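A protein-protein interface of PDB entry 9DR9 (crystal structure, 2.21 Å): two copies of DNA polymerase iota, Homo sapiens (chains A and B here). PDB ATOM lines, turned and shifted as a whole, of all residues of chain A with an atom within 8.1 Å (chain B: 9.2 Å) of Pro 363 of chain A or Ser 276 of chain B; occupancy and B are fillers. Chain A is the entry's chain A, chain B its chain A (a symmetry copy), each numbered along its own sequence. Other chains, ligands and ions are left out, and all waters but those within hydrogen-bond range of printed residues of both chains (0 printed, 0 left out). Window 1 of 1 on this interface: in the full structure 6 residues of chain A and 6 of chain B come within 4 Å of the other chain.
Of the 19 printed residues of chain B, 3 touch a printed residue of chain A.
Printed residues of chain B that touch a printed residue of chain A: Glu 270, Ile 275 and Ser 276.
Hydrophobic or aromatic side chains of chain B that line the printed part of chain A: Ile 275.
Of the 19 printed residues of chain A, 3 touch a printed residue of chain B.
Among the printed residues, 4 pairs touch across the chains.
No position is printed for both chains.
Of the 4 pairs that touch across the chains among the printed residues, none has its exchanged pair printed and touching as well.
The side-chain amide oxygen (OE1) of Gln 279 of chain B lies close to the side-chain carboxylate (OE2) of Glu 270 of chain B (3.3 Å).
No residue of chain B comes within 4 Å of Cys 362 of chain A.
Pro 363 of chain A touches just one residue of chain B: Ser 276.
Pro 365 of chain A touches none of the printed residues of chain B.
Of the printed residues of chain B, Lys 389 of chain A touches Glu 270 (2.9 Å) and Ile 275 (3.7 Å).
Of the printed residues of chain B, Leu 390 of chain A touches Ile 275.
Of the printed residues of chain A, Glu 270 of chain B touches Lys 389 (2.9 Å).
Gly 274 of chain B touches none of the printed residues of chain A.
Of the printed residues of chain A, Ile 275 of chain B touches Lys 389 and Leu 390.
Of chain A, only Pro 363 (3.2 Å) comes within 4 Å of Ser 276 of chain B.
The side-chain carboxylate (OE1) of Glu 270 of chain B is in salt-bridge range of the side-chain amino group (NZ) of Lys 389 of chain A, at 2.9 Å.
Among the printed residues, pairs that only touch across the chains: Leu 390 of chain A with Ile 275 of chain B (3.2 Å), Pro 363 of chain A with Ser 276 of chain B (3.2 Å) and Lys 389 of chain A with Ile 275 of chain B (3.7 Å).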
ATOM      1  N   PRO A 339      19.512  -7.261 -35.114  1.00  0.00           N
ATOM      2  CA  PRO A 339      19.410  -6.526 -33.849  1.00  0.00           C
ATOM      3  C   PRO A 339      18.003  -6.606 -33.266  1.00  0.00           C
ATOM      4  O   PRO A 339      17.004  -6.729 -33.977  1.00  0.00           O
ATOM      5  CB  PRO A 339      19.752  -5.086 -34.244  1.00  0.00           C
ATOM      6  CG  PRO A 339      19.368  -5.010 -35.656  1.00  0.00           C
ATOM      7  CD  PRO A 339      19.582  -6.357 -36.276  1.00  0.00           C
ATOM      8  N   HIS A 340      17.901  -6.610 -31.956  1.00  0.00           N
ATOM      9  CA  HIS A 340      16.564  -6.565 -31.383  1.00  0.00           C
ATOM     10  C   HIS A 340      16.319  -5.315 -30.564  1.00  0.00           C
ATOM     11  O   HIS A 340      15.461  -5.335 -29.666  1.00  0.00           O
ATOM     12  CB  HIS A 340      16.258  -7.775 -30.529  1.00  0.00           C
ATOM     13  CG  HIS A 340      16.142  -9.055 -31.288  1.00  0.00           C
ATOM     14  ND1 HIS A 340      16.987  -9.384 -32.327  1.00  0.00           N
ATOM     15  CD2 HIS A 340      15.401 -10.161 -31.041  1.00  0.00           C
ATOM     16  CE1 HIS A 340      16.716 -10.610 -32.737  1.00  0.00           C
ATOM     17  NE2 HIS A 340      15.768 -11.108 -31.964  1.00  0.00           N
ATOM     18  N   THR A 341      17.159  -4.308 -30.716  1.00  0.00           N
ATOM     19  CA  THR A 341      16.971  -3.059 -30.014  1.00  0.00           C
ATOM     20  C   THR A 341      17.463  -1.942 -30.902  1.00  0.00           C
ATOM     21  O   THR A 341      18.421  -2.097 -31.663  1.00  0.00           O
ATOM     22  CB  THR A 341      17.722  -3.017 -28.686  1.00  0.00           C
ATOM     23  OG1 THR A 341      17.381  -4.172 -27.914  1.00  0.00           O
ATOM     24  CG2 THR A 341      17.377  -1.748 -27.962  1.00  0.00           C
ATOM     25  N   VAL A 342      16.750  -0.825 -30.828  1.00  0.00           N
ATOM     26  CA  VAL A 342      17.180   0.401 -31.471  1.00  0.00           C
ATOM     27  C   VAL A 342      17.224   1.486 -30.406  1.00  0.00           C
ATOM     28  O   VAL A 342      16.415   1.495 -29.467  1.00  0.00           O
ATOM     29  CB  VAL A 342      16.242   0.801 -32.625  1.00  0.00           C
ATOM     30  CG1 VAL A 342      15.027   1.489 -32.052  1.00  0.00           C
ATOM     31  CG2 VAL A 342      16.970   1.604 -33.678  1.00  0.00           C
ATOM     32  N   ARG A 343      18.178   2.407 -30.568  1.00  0.00           N
ATOM     33  CA  ARG A 343      18.407   3.519 -29.656  1.00  0.00           C
ATOM     34  C   ARG A 343      18.668   4.789 -30.463  1.00  0.00           C
ATOM     35  O   ARG A 343      19.402   4.783 -31.457  1.00  0.00           O
ATOM     36  CB  ARG A 343      19.586   3.155 -28.714  1.00  0.00           C
ATOM     37  CG  ARG A 343      20.024   4.293 -27.804  1.00  0.00           C
ATOM     38  CD  ARG A 343      21.192   4.004 -26.794  1.00  0.00           C
ATOM     39  NE  ARG A 343      21.083   2.752 -26.060  1.00  0.00           N
ATOM     40  CZ  ARG A 343      21.890   1.703 -26.198  1.00  0.00           C
ATOM     41  NH1 ARG A 343      22.920   1.708 -27.041  1.00  0.00           N
ATOM     42  NH2 ARG A 343      21.631   0.601 -25.499  1.00  0.00           N
ATOM     43  N   GLN A 361      15.749   4.083 -26.039  1.00  0.00           N
ATOM     44  CA  GLN A 361      15.755   2.853 -26.819  1.00  0.00           C
ATOM     45  C   GLN A 361      14.412   2.131 -26.672  1.00  0.00           C
ATOM     46  O   GLN A 361      13.584   2.461 -25.828  1.00  0.00           O
ATOM     47  CB  GLN A 361      16.901   1.920 -26.377  1.00  0.00           C
ATOM     48  CG  GLN A 361      16.867   1.599 -24.911  1.00  0.00           C
ATOM     49  CD  GLN A 361      18.041   0.803 -24.442  1.00  0.00           C
ATOM     50  OE1 GLN A 361      19.174   1.283 -24.265  1.00  0.00           O
ATOM     51  NE2 GLN A 361      17.781  -0.485 -24.301  1.00  0.00           N
ATOM     52  N   CYS A 362      14.205   1.121 -27.497  1.00  0.00           N
ATOM     53  CA  CYS A 362      13.012   0.286 -27.426  1.00  0.00           C
ATOM     54  C   CYS A 362      13.304  -0.955 -28.245  1.00  0.00           C
ATOM     55  O   CYS A 362      14.074  -0.892 -29.218  1.00  0.00           O
ATOM     56  CB  CYS A 362      11.763   1.024 -27.969  1.00  0.00           C
ATOM     57  SG  CYS A 362      11.716   1.197 -29.769  1.00  0.00           S
ATOM     58  N   PRO A 363      12.669  -2.083 -27.912  1.00  0.00           N
ATOM     59  CA  PRO A 363      12.853  -3.288 -28.725  1.00  0.00           C
ATOM     60  C   PRO A 363      12.392  -3.097 -30.139  1.00  0.00           C
ATOM     61  O   PRO A 363      11.604  -2.208 -30.421  1.00  0.00           O
ATOM     62  CB  PRO A 363      11.942  -4.326 -28.062  1.00  0.00           C
ATOM     63  CG  PRO A 363      11.493  -3.801 -26.821  1.00  0.00           C
ATOM     64  CD  PRO A 363      11.891  -2.354 -26.689  1.00  0.00           C
ATOM     65  N   ILE A 364      12.879  -3.925 -31.050  1.00  0.00           N
ATOM     66  CA  ILE A 364      12.467  -3.864 -32.448  1.00  0.00           C
ATOM     67  C   ILE A 364      11.376  -4.906 -32.656  1.00  0.00           C
ATOM     68  O   ILE A 364      11.649  -6.110 -32.469  1.00  0.00           O
ATOM     69  CB  ILE A 364      13.644  -4.123 -33.395  1.00  0.00           C
ATOM     70  CG1 ILE A 364      14.802  -3.198 -33.102  1.00  0.00           C
ATOM     71  CG2 ILE A 364      13.249  -3.947 -34.845  1.00  0.00           C
ATOM     72  CD1 ILE A 364      15.940  -3.247 -34.105  1.00  0.00           C
ATOM     73  N   PRO A 365      10.153  -4.519 -33.072  1.00  0.00           N
ATOM     74  CA  PRO A 365       9.086  -5.511 -33.243  1.00  0.00           C
ATOM     75  C   PRO A 365       9.560  -6.729 -34.021  1.00  0.00           C
ATOM     76  O   PRO A 365      10.458  -6.644 -34.864  1.00  0.00           O
ATOM     77  CB  PRO A 365       8.011  -4.740 -34.019  1.00  0.00           C
ATOM     78  CG  PRO A 365       8.239  -3.320 -33.691  1.00  0.00           C
ATOM     79  CD  PRO A 365       9.614  -3.142 -33.134  1.00  0.00           C
ATOM     80  N   SER A 366       8.961  -7.880 -33.688  1.00  0.00           N
ATOM     81  CA  SER A 366       9.335  -9.152 -34.307  1.00  0.00           C
ATOM     82  C   SER A 366       9.220  -9.077 -35.822  1.00  0.00           C
ATOM     83  O   SER A 366      10.141  -9.468 -36.550  1.00  0.00           O
ATOM     84  CB  SER A 366       8.491 -10.294 -33.731  1.00  0.00           C
ATOM     85  OG  SER A 366       8.513 -10.219 -32.315  1.00  0.00           O
ATOM     86  N   VAL A 368       9.416  -6.686 -37.795  1.00  0.00           N
ATOM     87  CA  VAL A 368      10.384  -5.762 -38.356  1.00  0.00           C
ATOM     88  C   VAL A 368      11.743  -6.452 -38.500  1.00  0.00           C
ATOM     89  O   VAL A 368      12.340  -6.363 -39.588  1.00  0.00           O
ATOM     90  CB  VAL A 368      10.524  -4.476 -37.516  1.00  0.00           C
ATOM     91  CG1 VAL A 368      11.604  -3.538 -38.115  1.00  0.00           C
ATOM     92  CG2 VAL A 368       9.183  -3.725 -37.558  1.00  0.00           C
ATOM     93  N   ILE A 369      12.158  -7.251 -37.494  1.00  0.00           N
ATOM     94  CA  ILE A 369      13.414  -8.003 -37.493  1.00  0.00           C
ATOM     95  C   ILE A 369      13.580  -8.718 -38.810  1.00  0.00           C
ATOM     96  O   ILE A 369      14.718  -8.788 -39.346  1.00  0.00           O
ATOM     97  CB  ILE A 369      13.383  -8.922 -36.248  1.00  0.00           C
ATOM     98  CG1 ILE A 369      13.412  -7.957 -35.081  1.00  0.00           C
ATOM     99  CG2 ILE A 369      14.562  -9.793 -36.156  1.00  0.00           C
ATOM    100  CD1 ILE A 369      13.779  -8.499 -33.721  1.00  0.00           C
ATOM    101  N   MET A 383      10.785   1.619 -39.208  1.00  0.00           N
ATOM    102  CA  MET A 383      11.870   2.034 -38.320  1.00  0.00           C
ATOM    103  C   MET A 383      11.854   3.532 -38.024  1.00  0.00           C
ATOM    104  O   MET A 383      12.227   3.949 -36.922  1.00  0.00           O
ATOM    105  CB  MET A 383      13.247   1.627 -38.869  1.00  0.00           C
ATOM    106  CG  MET A 383      13.581   0.120 -38.793  1.00  0.00           C
ATOM    107  SD  MET A 383      13.473  -0.656 -37.157  1.00  0.00           S
ATOM    108  CE  MET A 383      14.329   0.566 -36.159  1.00  0.00           C
ATOM    109  N   ILE A 386       9.032   4.569 -35.328  1.00  0.00           N
ATOM    110  CA  ILE A 386       9.594   4.151 -34.055  1.00  0.00           C
ATOM    111  C   ILE A 386      10.589   5.222 -33.623  1.00  0.00           C
ATOM    112  O   ILE A 386      10.532   5.717 -32.494  1.00  0.00           O
ATOM    113  CB  ILE A 386      10.261   2.764 -34.186  1.00  0.00           C
ATOM    114  CG1 ILE A 386       9.305   1.553 -34.148  1.00  0.00           C
ATOM    115  CG2 ILE A 386      11.336   2.687 -33.106  1.00  0.00           C
ATOM    116  CD1 ILE A 386       9.780   0.503 -35.263  1.00  0.00           C
ATOM    117  N   LYS A 389       8.985   8.592 -32.682  1.00  0.00           N
ATOM    118  CA  LYS A 389       8.401   8.498 -31.345  1.00  0.00           C
ATOM    119  C   LYS A 389       9.475   8.603 -30.285  1.00  0.00           C
ATOM    120  O   LYS A 389       9.286   9.325 -29.307  1.00  0.00           O
ATOM    121  CB  LYS A 389       7.615   7.198 -31.208  1.00  0.00           C
ATOM    122  CG  LYS A 389       6.384   7.137 -32.154  1.00  0.00           C
ATOM    123  CD  LYS A 389       5.914   5.709 -32.349  1.00  0.00           C
ATOM    124  CE  LYS A 389       4.959   5.649 -33.621  1.00  0.00           C
ATOM    125  NZ  LYS A 389       4.201   4.385 -33.703  1.00  0.00           N
ATOM    126  N   LEU A 390      10.603   7.902 -30.443  1.00  0.00           N
ATOM    127  CA  LEU A 390      11.700   8.090 -29.500  1.00  0.00           C
ATOM    128  C   LEU A 390      12.192   9.520 -29.540  1.00  0.00           C
ATOM    129  O   LEU A 390      12.587  10.092 -28.520  1.00  0.00           O
ATOM    130  CB  LEU A 390      12.845   7.143 -29.832  1.00  0.00           C
ATOM    131  CG  LEU A 390      12.477   5.662 -29.770  1.00  0.00           C
ATOM    132  CD1 LEU A 390      13.673   4.759 -30.085  1.00  0.00           C
ATOM    133  CD2 LEU A 390      11.876   5.280 -28.449  1.00  0.00           C
ATOM    134  N   CYS A 411      21.504  -2.404 -31.258  1.00  0.00           N
ATOM    135  CA  CYS A 411      22.125  -3.330 -30.333  1.00  0.00           C
ATOM    136  C   CYS A 411      21.131  -4.460 -30.068  1.00  0.00           C
ATOM    137  O   CYS A 411      20.093  -4.595 -30.726  1.00  0.00           O
ATOM    138  CB  CYS A 411      22.607  -2.602 -29.072  1.00  0.00           C
ATOM    139  SG  CYS A 411      21.298  -1.737 -28.253  1.00  0.00           S
ATOM    140  N   ASN A 412      21.518  -5.277 -29.101  1.00  0.00           N
ATOM    141  CA  ASN A 412      20.833  -6.466 -28.637  1.00  0.00           C
ATOM    142  C   ASN A 412      20.849  -7.490 -29.770  1.00  0.00           C
ATOM    143  O   ASN A 412      19.800  -7.938 -30.252  1.00  0.00           O
ATOM    144  CB  ASN A 412      19.388  -6.262 -28.276  1.00  0.00           C
ATOM    145  CG  ASN A 412      18.996  -7.167 -27.154  1.00  0.00           C
ATOM    146  OD1 ASN A 412      19.291  -8.387 -27.094  1.00  0.00           O
ATOM    147  ND2 ASN A 412      18.209  -6.580 -26.270  1.00  0.00           N
ATOM    148  N   GLY B 241       1.764  -9.209 -17.421  1.00  0.00           N
ATOM    149  CA  GLY B 241       2.512  -8.185 -18.122  1.00  0.00           C
ATOM    150  C   GLY B 241       1.995  -6.791 -17.865  1.00  0.00           C
ATOM    151  O   GLY B 241       2.736  -5.822 -18.074  1.00  0.00           O
ATOM    152  N   LYS B 245       2.241  -0.557 -11.809  1.00  0.00           N
ATOM    153  CA  LYS B 245       2.335   0.761 -12.447  1.00  0.00           C
ATOM    154  C   LYS B 245       1.449   0.884 -13.692  1.00  0.00           C
ATOM    155  O   LYS B 245       0.709   1.861 -13.839  1.00  0.00           O
ATOM    156  CB  LYS B 245       3.796   1.044 -12.832  1.00  0.00           C
ATOM    157  CG  LYS B 245       4.137   2.440 -13.302  1.00  0.00           C
ATOM    158  CD  LYS B 245       3.911   2.553 -14.779  1.00  0.00           C
ATOM    159  CE  LYS B 245       5.016   2.000 -15.624  1.00  0.00           C
ATOM    160  NZ  LYS B 245       4.651   1.270 -16.887  1.00  0.00           N
ATOM    161  N   THR B 246       1.518  -0.096 -14.601  1.00  0.00           N
ATOM    162  CA  THR B 246       0.821   0.011 -15.884  1.00  0.00           C
ATOM    163  C   THR B 246      -0.688   0.033 -15.712  1.00  0.00           C
ATOM    164  O   THR B 246      -1.389   0.840 -16.340  1.00  0.00           O
ATOM    165  CB  THR B 246       1.251  -1.143 -16.774  1.00  0.00           C
ATOM    166  OG1 THR B 246       2.662  -1.311 -16.612  1.00  0.00           O
ATOM    167  CG2 THR B 246       0.982  -0.761 -18.204  1.00  0.00           C
ATOM    168  N   LEU B 269      -1.617   5.663 -26.521  1.00  0.00           N
ATOM    169  CA  LEU B 269      -1.002   4.653 -25.681  1.00  0.00           C
ATOM    170  C   LEU B 269       0.509   4.688 -25.815  1.00  0.00           C
ATOM    171  O   LEU B 269       1.223   4.624 -24.814  1.00  0.00           O
ATOM    172  CB  LEU B 269      -1.565   3.279 -26.035  1.00  0.00           C
ATOM    173  CG  LEU B 269      -1.414   2.165 -24.993  1.00  0.00           C
ATOM    174  CD1 LEU B 269      -2.200   2.469 -23.756  1.00  0.00           C
ATOM    175  CD2 LEU B 269      -1.895   0.812 -25.593  1.00  0.00           C
ATOM    176  N   GLU B 270       1.022   4.799 -27.044  1.00  0.00           N
ATOM    177  CA  GLU B 270       2.468   4.890 -27.222  1.00  0.00           C
ATOM    178  C   GLU B 270       3.026   6.106 -26.490  1.00  0.00           C
ATOM    179  O   GLU B 270       4.040   6.016 -25.791  1.00  0.00           O
ATOM    180  CB  GLU B 270       2.829   4.957 -28.703  1.00  0.00           C
ATOM    181  CG  GLU B 270       2.719   3.631 -29.448  1.00  0.00           C
ATOM    182  CD  GLU B 270       2.720   3.856 -30.960  1.00  0.00           C
ATOM    183  OE1 GLU B 270       2.706   5.053 -31.361  1.00  0.00           O
ATOM    184  OE2 GLU B 270       2.692   2.866 -31.735  1.00  0.00           O
ATOM    185  N   LYS B 271       2.387   7.262 -26.658  1.00  0.00           N
ATOM    186  CA  LYS B 271       2.932   8.493 -26.090  1.00  0.00           C
ATOM    187  C   LYS B 271       2.849   8.505 -24.580  1.00  0.00           C
ATOM    188  O   LYS B 271       3.601   9.218 -23.909  1.00  0.00           O
ATOM    189  CB  LYS B 271       2.199   9.700 -26.671  1.00  0.00           C
ATOM    190  CG  LYS B 271       2.654  11.040 -26.170  1.00  0.00           C
ATOM    191  CD  LYS B 271       2.382  12.128 -27.234  1.00  0.00           C
ATOM    192  CE  LYS B 271       1.003  12.787 -27.047  1.00  0.00           C
ATOM    193  NZ  LYS B 271       0.253  12.816 -28.321  1.00  0.00           N
ATOM    194  N   GLU B 272       1.957   7.729 -24.021  1.00  0.00           N
ATOM    195  CA  GLU B 272       1.820   7.767 -22.581  1.00  0.00           C
ATOM    196  C   GLU B 272       2.689   6.743 -21.872  1.00  0.00           C
ATOM    197  O   GLU B 272       3.003   6.907 -20.683  1.00  0.00           O
ATOM    198  CB  GLU B 272       0.365   7.517 -22.232  1.00  0.00           C
ATOM    199  CG  GLU B 272       0.149   6.951 -20.839  1.00  0.00           C
ATOM    200  CD  GLU B 272       0.113   7.990 -19.757  1.00  0.00           C
ATOM    201  OE1 GLU B 272      -0.056   9.198 -20.118  1.00  0.00           O
ATOM    202  OE2 GLU B 272       0.139   7.579 -18.572  1.00  0.00           O
ATOM    203  N   LEU B 273       2.931   5.603 -22.503  1.00  0.00           N
ATOM    204  CA  LEU B 273       3.655   4.561 -21.796  1.00  0.00           C
ATOM    205  C   LEU B 273       4.916   4.089 -22.455  1.00  0.00           C
ATOM    206  O   LEU B 273       5.786   3.517 -21.760  1.00  0.00           O
ATOM    207  CB  LEU B 273       2.761   3.326 -21.635  1.00  0.00           C
ATOM    208  CG  LEU B 273       1.396   3.452 -20.953  1.00  0.00           C
ATOM    209  CD1 LEU B 273       0.561   2.207 -21.302  1.00  0.00           C
ATOM    210  CD2 LEU B 273       1.469   3.644 -19.462  1.00  0.00           C
ATOM    211  N   GLY B 274       5.065   4.405 -23.722  1.00  0.00           N
ATOM    212  CA  GLY B 274       6.202   3.980 -24.480  1.00  0.00           C
ATOM    213  C   GLY B 274       5.845   3.097 -25.647  1.00  0.00           C
ATOM    214  O   GLY B 274       4.874   2.339 -25.640  1.00  0.00           O
ATOM    215  N   ILE B 275       6.653   3.236 -26.684  1.00  0.00           N
ATOM    216  CA  ILE B 275       6.386   2.372 -27.805  1.00  0.00           C
ATOM    217  C   ILE B 275       6.422   0.923 -27.348  1.00  0.00           C
ATOM    218  O   ILE B 275       5.566   0.126 -27.741  1.00  0.00           O
ATOM    219  CB  ILE B 275       7.302   2.628 -29.018  1.00  0.00           C
ATOM    220  CG1 ILE B 275       7.560   4.108 -29.243  1.00  0.00           C
ATOM    221  CG2 ILE B 275       6.625   1.919 -30.167  1.00  0.00           C
ATOM    222  CD1 ILE B 275       8.810   4.537 -28.533  1.00  0.00           C
ATOM    223  N   SER B 276       7.330   0.588 -26.432  1.00  0.00           N
ATOM    224  CA  SER B 276       7.501  -0.792 -26.002  1.00  0.00           C
ATOM    225  C   SER B 276       6.307  -1.279 -25.194  1.00  0.00           C
ATOM    226  O   SER B 276       5.662  -2.275 -25.540  1.00  0.00           O
ATOM    227  CB  SER B 276       8.798  -0.907 -25.213  1.00  0.00           C
ATOM    228  OG  SER B 276       9.111  -2.269 -25.046  1.00  0.00           O
ATOM    229  N   VAL B 277       5.994  -0.587 -24.109  1.00  0.00           N
ATOM    230  CA  VAL B 277       4.922  -1.050 -23.243  1.00  0.00           C
ATOM    231  C   VAL B 277       3.605  -1.088 -23.985  1.00  0.00           C
ATOM    232  O   VAL B 277       2.850  -2.063 -23.902  1.00  0.00           O
ATOM    233  CB  VAL B 277       4.841  -0.164 -21.999  1.00  0.00           C
ATOM    234  CG1 VAL B 277       3.530  -0.403 -21.318  1.00  0.00           C
ATOM    235  CG2 VAL B 277       5.997  -0.522 -21.088  1.00  0.00           C
ATOM    236  N   ALA B 278       3.317  -0.032 -24.727  1.00  0.00           N
ATOM    237  CA  ALA B 278       2.019   0.104 -25.367  1.00  0.00           C
ATOM    238  C   ALA B 278       1.793  -1.004 -26.373  1.00  0.00           C
ATOM    239  O   ALA B 278       0.782  -1.712 -26.348  1.00  0.00           O
ATOM    240  CB  ALA B 278       1.948   1.451 -26.060  1.00  0.00           C
ATOM    241  N   GLN B 279       2.728  -1.137 -27.288  1.00  0.00           N
ATOM    242  CA  GLN B 279       2.601  -2.090 -28.371  1.00  0.00           C
ATOM    243  C   GLN B 279       2.503  -3.509 -27.876  1.00  0.00           C
ATOM    244  O   GLN B 279       1.874  -4.336 -28.535  1.00  0.00           O
ATOM    245  CB  GLN B 279       3.708  -1.821 -29.364  1.00  0.00           C
ATOM    246  CG  GLN B 279       3.052  -1.243 -30.685  1.00  0.00           C
ATOM    247  CD  GLN B 279       3.995  -1.116 -31.851  1.00  0.00           C
ATOM    248  OE1 GLN B 279       4.291   0.000 -32.303  1.00  0.00           O
ATOM    249  NE2 GLN B 279       4.368  -2.231 -32.425  1.00  0.00           N
ATOM    250  N   ARG B 280       3.052  -3.785 -26.703  1.00  0.00           N
ATOM    251  CA  ARG B 280       3.095  -5.140 -26.182  1.00  0.00           C
ATOM    252  C   ARG B 280       1.849  -5.472 -25.346  1.00  0.00           C
ATOM    253  O   ARG B 280       1.341  -6.597 -25.375  1.00  0.00           O
ATOM    254  CB  ARG B 280       4.332  -5.255 -25.334  1.00  0.00           C
ATOM    255  CG  ARG B 280       4.342  -6.352 -24.337  1.00  0.00           C
ATOM    256  CD  ARG B 280       4.575  -7.796 -24.898  1.00  0.00           C
ATOM    257  NE  ARG B 280       4.360  -8.850 -23.897  1.00  0.00           N
ATOM    258  CZ  ARG B 280       4.309 -10.145 -24.187  1.00  0.00           C
ATOM    259  NH1 ARG B 280       4.472 -10.575 -25.424  1.00  0.00           N
ATOM    260  NH2 ARG B 280       4.169 -11.037 -23.204  1.00  0.00           N
ATOM    261  N   ILE B 281       1.384  -4.535 -24.520  1.00  0.00           N
ATOM    262  CA  ILE B 281       0.193  -4.846 -23.733  1.00  0.00           C
ATOM    263  C   ILE B 281      -1.047  -4.760 -24.606  1.00  0.00           C
ATOM    264  O   ILE B 281      -2.039  -5.449 -24.341  1.00  0.00           O
ATOM    265  CB  ILE B 281       0.123  -3.958 -22.478  1.00  0.00           C
ATOM    266  CG1 ILE B 281      -0.234  -2.546 -22.883  1.00  0.00           C
ATOM    267  CG2 ILE B 281       1.405  -4.022 -21.708  1.00  0.00           C
ATOM    268  CD1 ILE B 281      -0.599  -1.690 -21.713  1.00  0.00           C
ATOM    269  N   GLN B 282      -1.027  -3.948 -25.674  1.00  0.00           N
ATOM    270  CA  GLN B 282      -2.216  -3.961 -26.530  1.00  0.00           C
ATOM    271  C   GLN B 282      -2.334  -5.239 -27.367  1.00  0.00           C
ATOM    272  O   GLN B 282      -3.450  -5.719 -27.602  1.00  0.00           O
ATOM    273  CB  GLN B 282      -2.278  -2.751 -27.468  1.00  0.00           C
ATOM    274  CG  GLN B 282      -3.645  -2.666 -28.235  1.00  0.00           C
ATOM    275  CD  GLN B 282      -3.893  -1.258 -28.790  1.00  0.00           C
ATOM    276  OE1 GLN B 282      -3.760  -0.270 -28.057  1.00  0.00           O
ATOM    277  NE2 GLN B 282      -4.342  -1.167 -30.049  1.00  0.00           N
ATOM    278  N   LYS B 283      -1.206  -5.801 -27.817  1.00  0.00           N
ATOM    279  CA  LYS B 283      -1.190  -7.147 -28.389  1.00  0.00           C
ATOM    280  C   LYS B 283      -1.719  -8.146 -27.373  1.00  0.00           C
ATOM    281  O   LYS B 283      -2.606  -8.955 -27.670  1.00  0.00           O
ATOM    282  CB  LYS B 283       0.247  -7.463 -28.840  1.00  0.00           C
ATOM    283  CG  LYS B 283       0.615  -6.943 -30.231  1.00  0.00           C
ATOM    284  CD  LYS B 283       1.891  -7.578 -30.940  1.00  0.00           C
ATOM    285  CE  LYS B 283       1.438  -8.034 -32.295  1.00  0.00           C
ATOM    286  NZ  LYS B 283       1.356  -6.877 -33.160  1.00  0.00           N
ATOM    287  N   LEU B 284      -1.224  -8.059 -26.140  1.00  0.00           N
ATOM    288  CA  LEU B 284      -1.724  -8.934 -25.087  1.00  0.00           C
ATOM    289  C   LEU B 284      -3.229  -8.808 -24.923  1.00  0.00           C
ATOM    290  O   LEU B 284      -3.917  -9.804 -24.674  1.00  0.00           O
ATOM    291  CB  LEU B 284      -1.024  -8.612 -23.773  1.00  0.00           C
ATOM    292  CG  LEU B 284       0.454  -8.991 -23.682  1.00  0.00           C
ATOM    293  CD1 LEU B 284       1.008  -8.454 -22.376  1.00  0.00           C
ATOM    294  CD2 LEU B 284       0.690 -10.501 -23.731  1.00  0.00           C
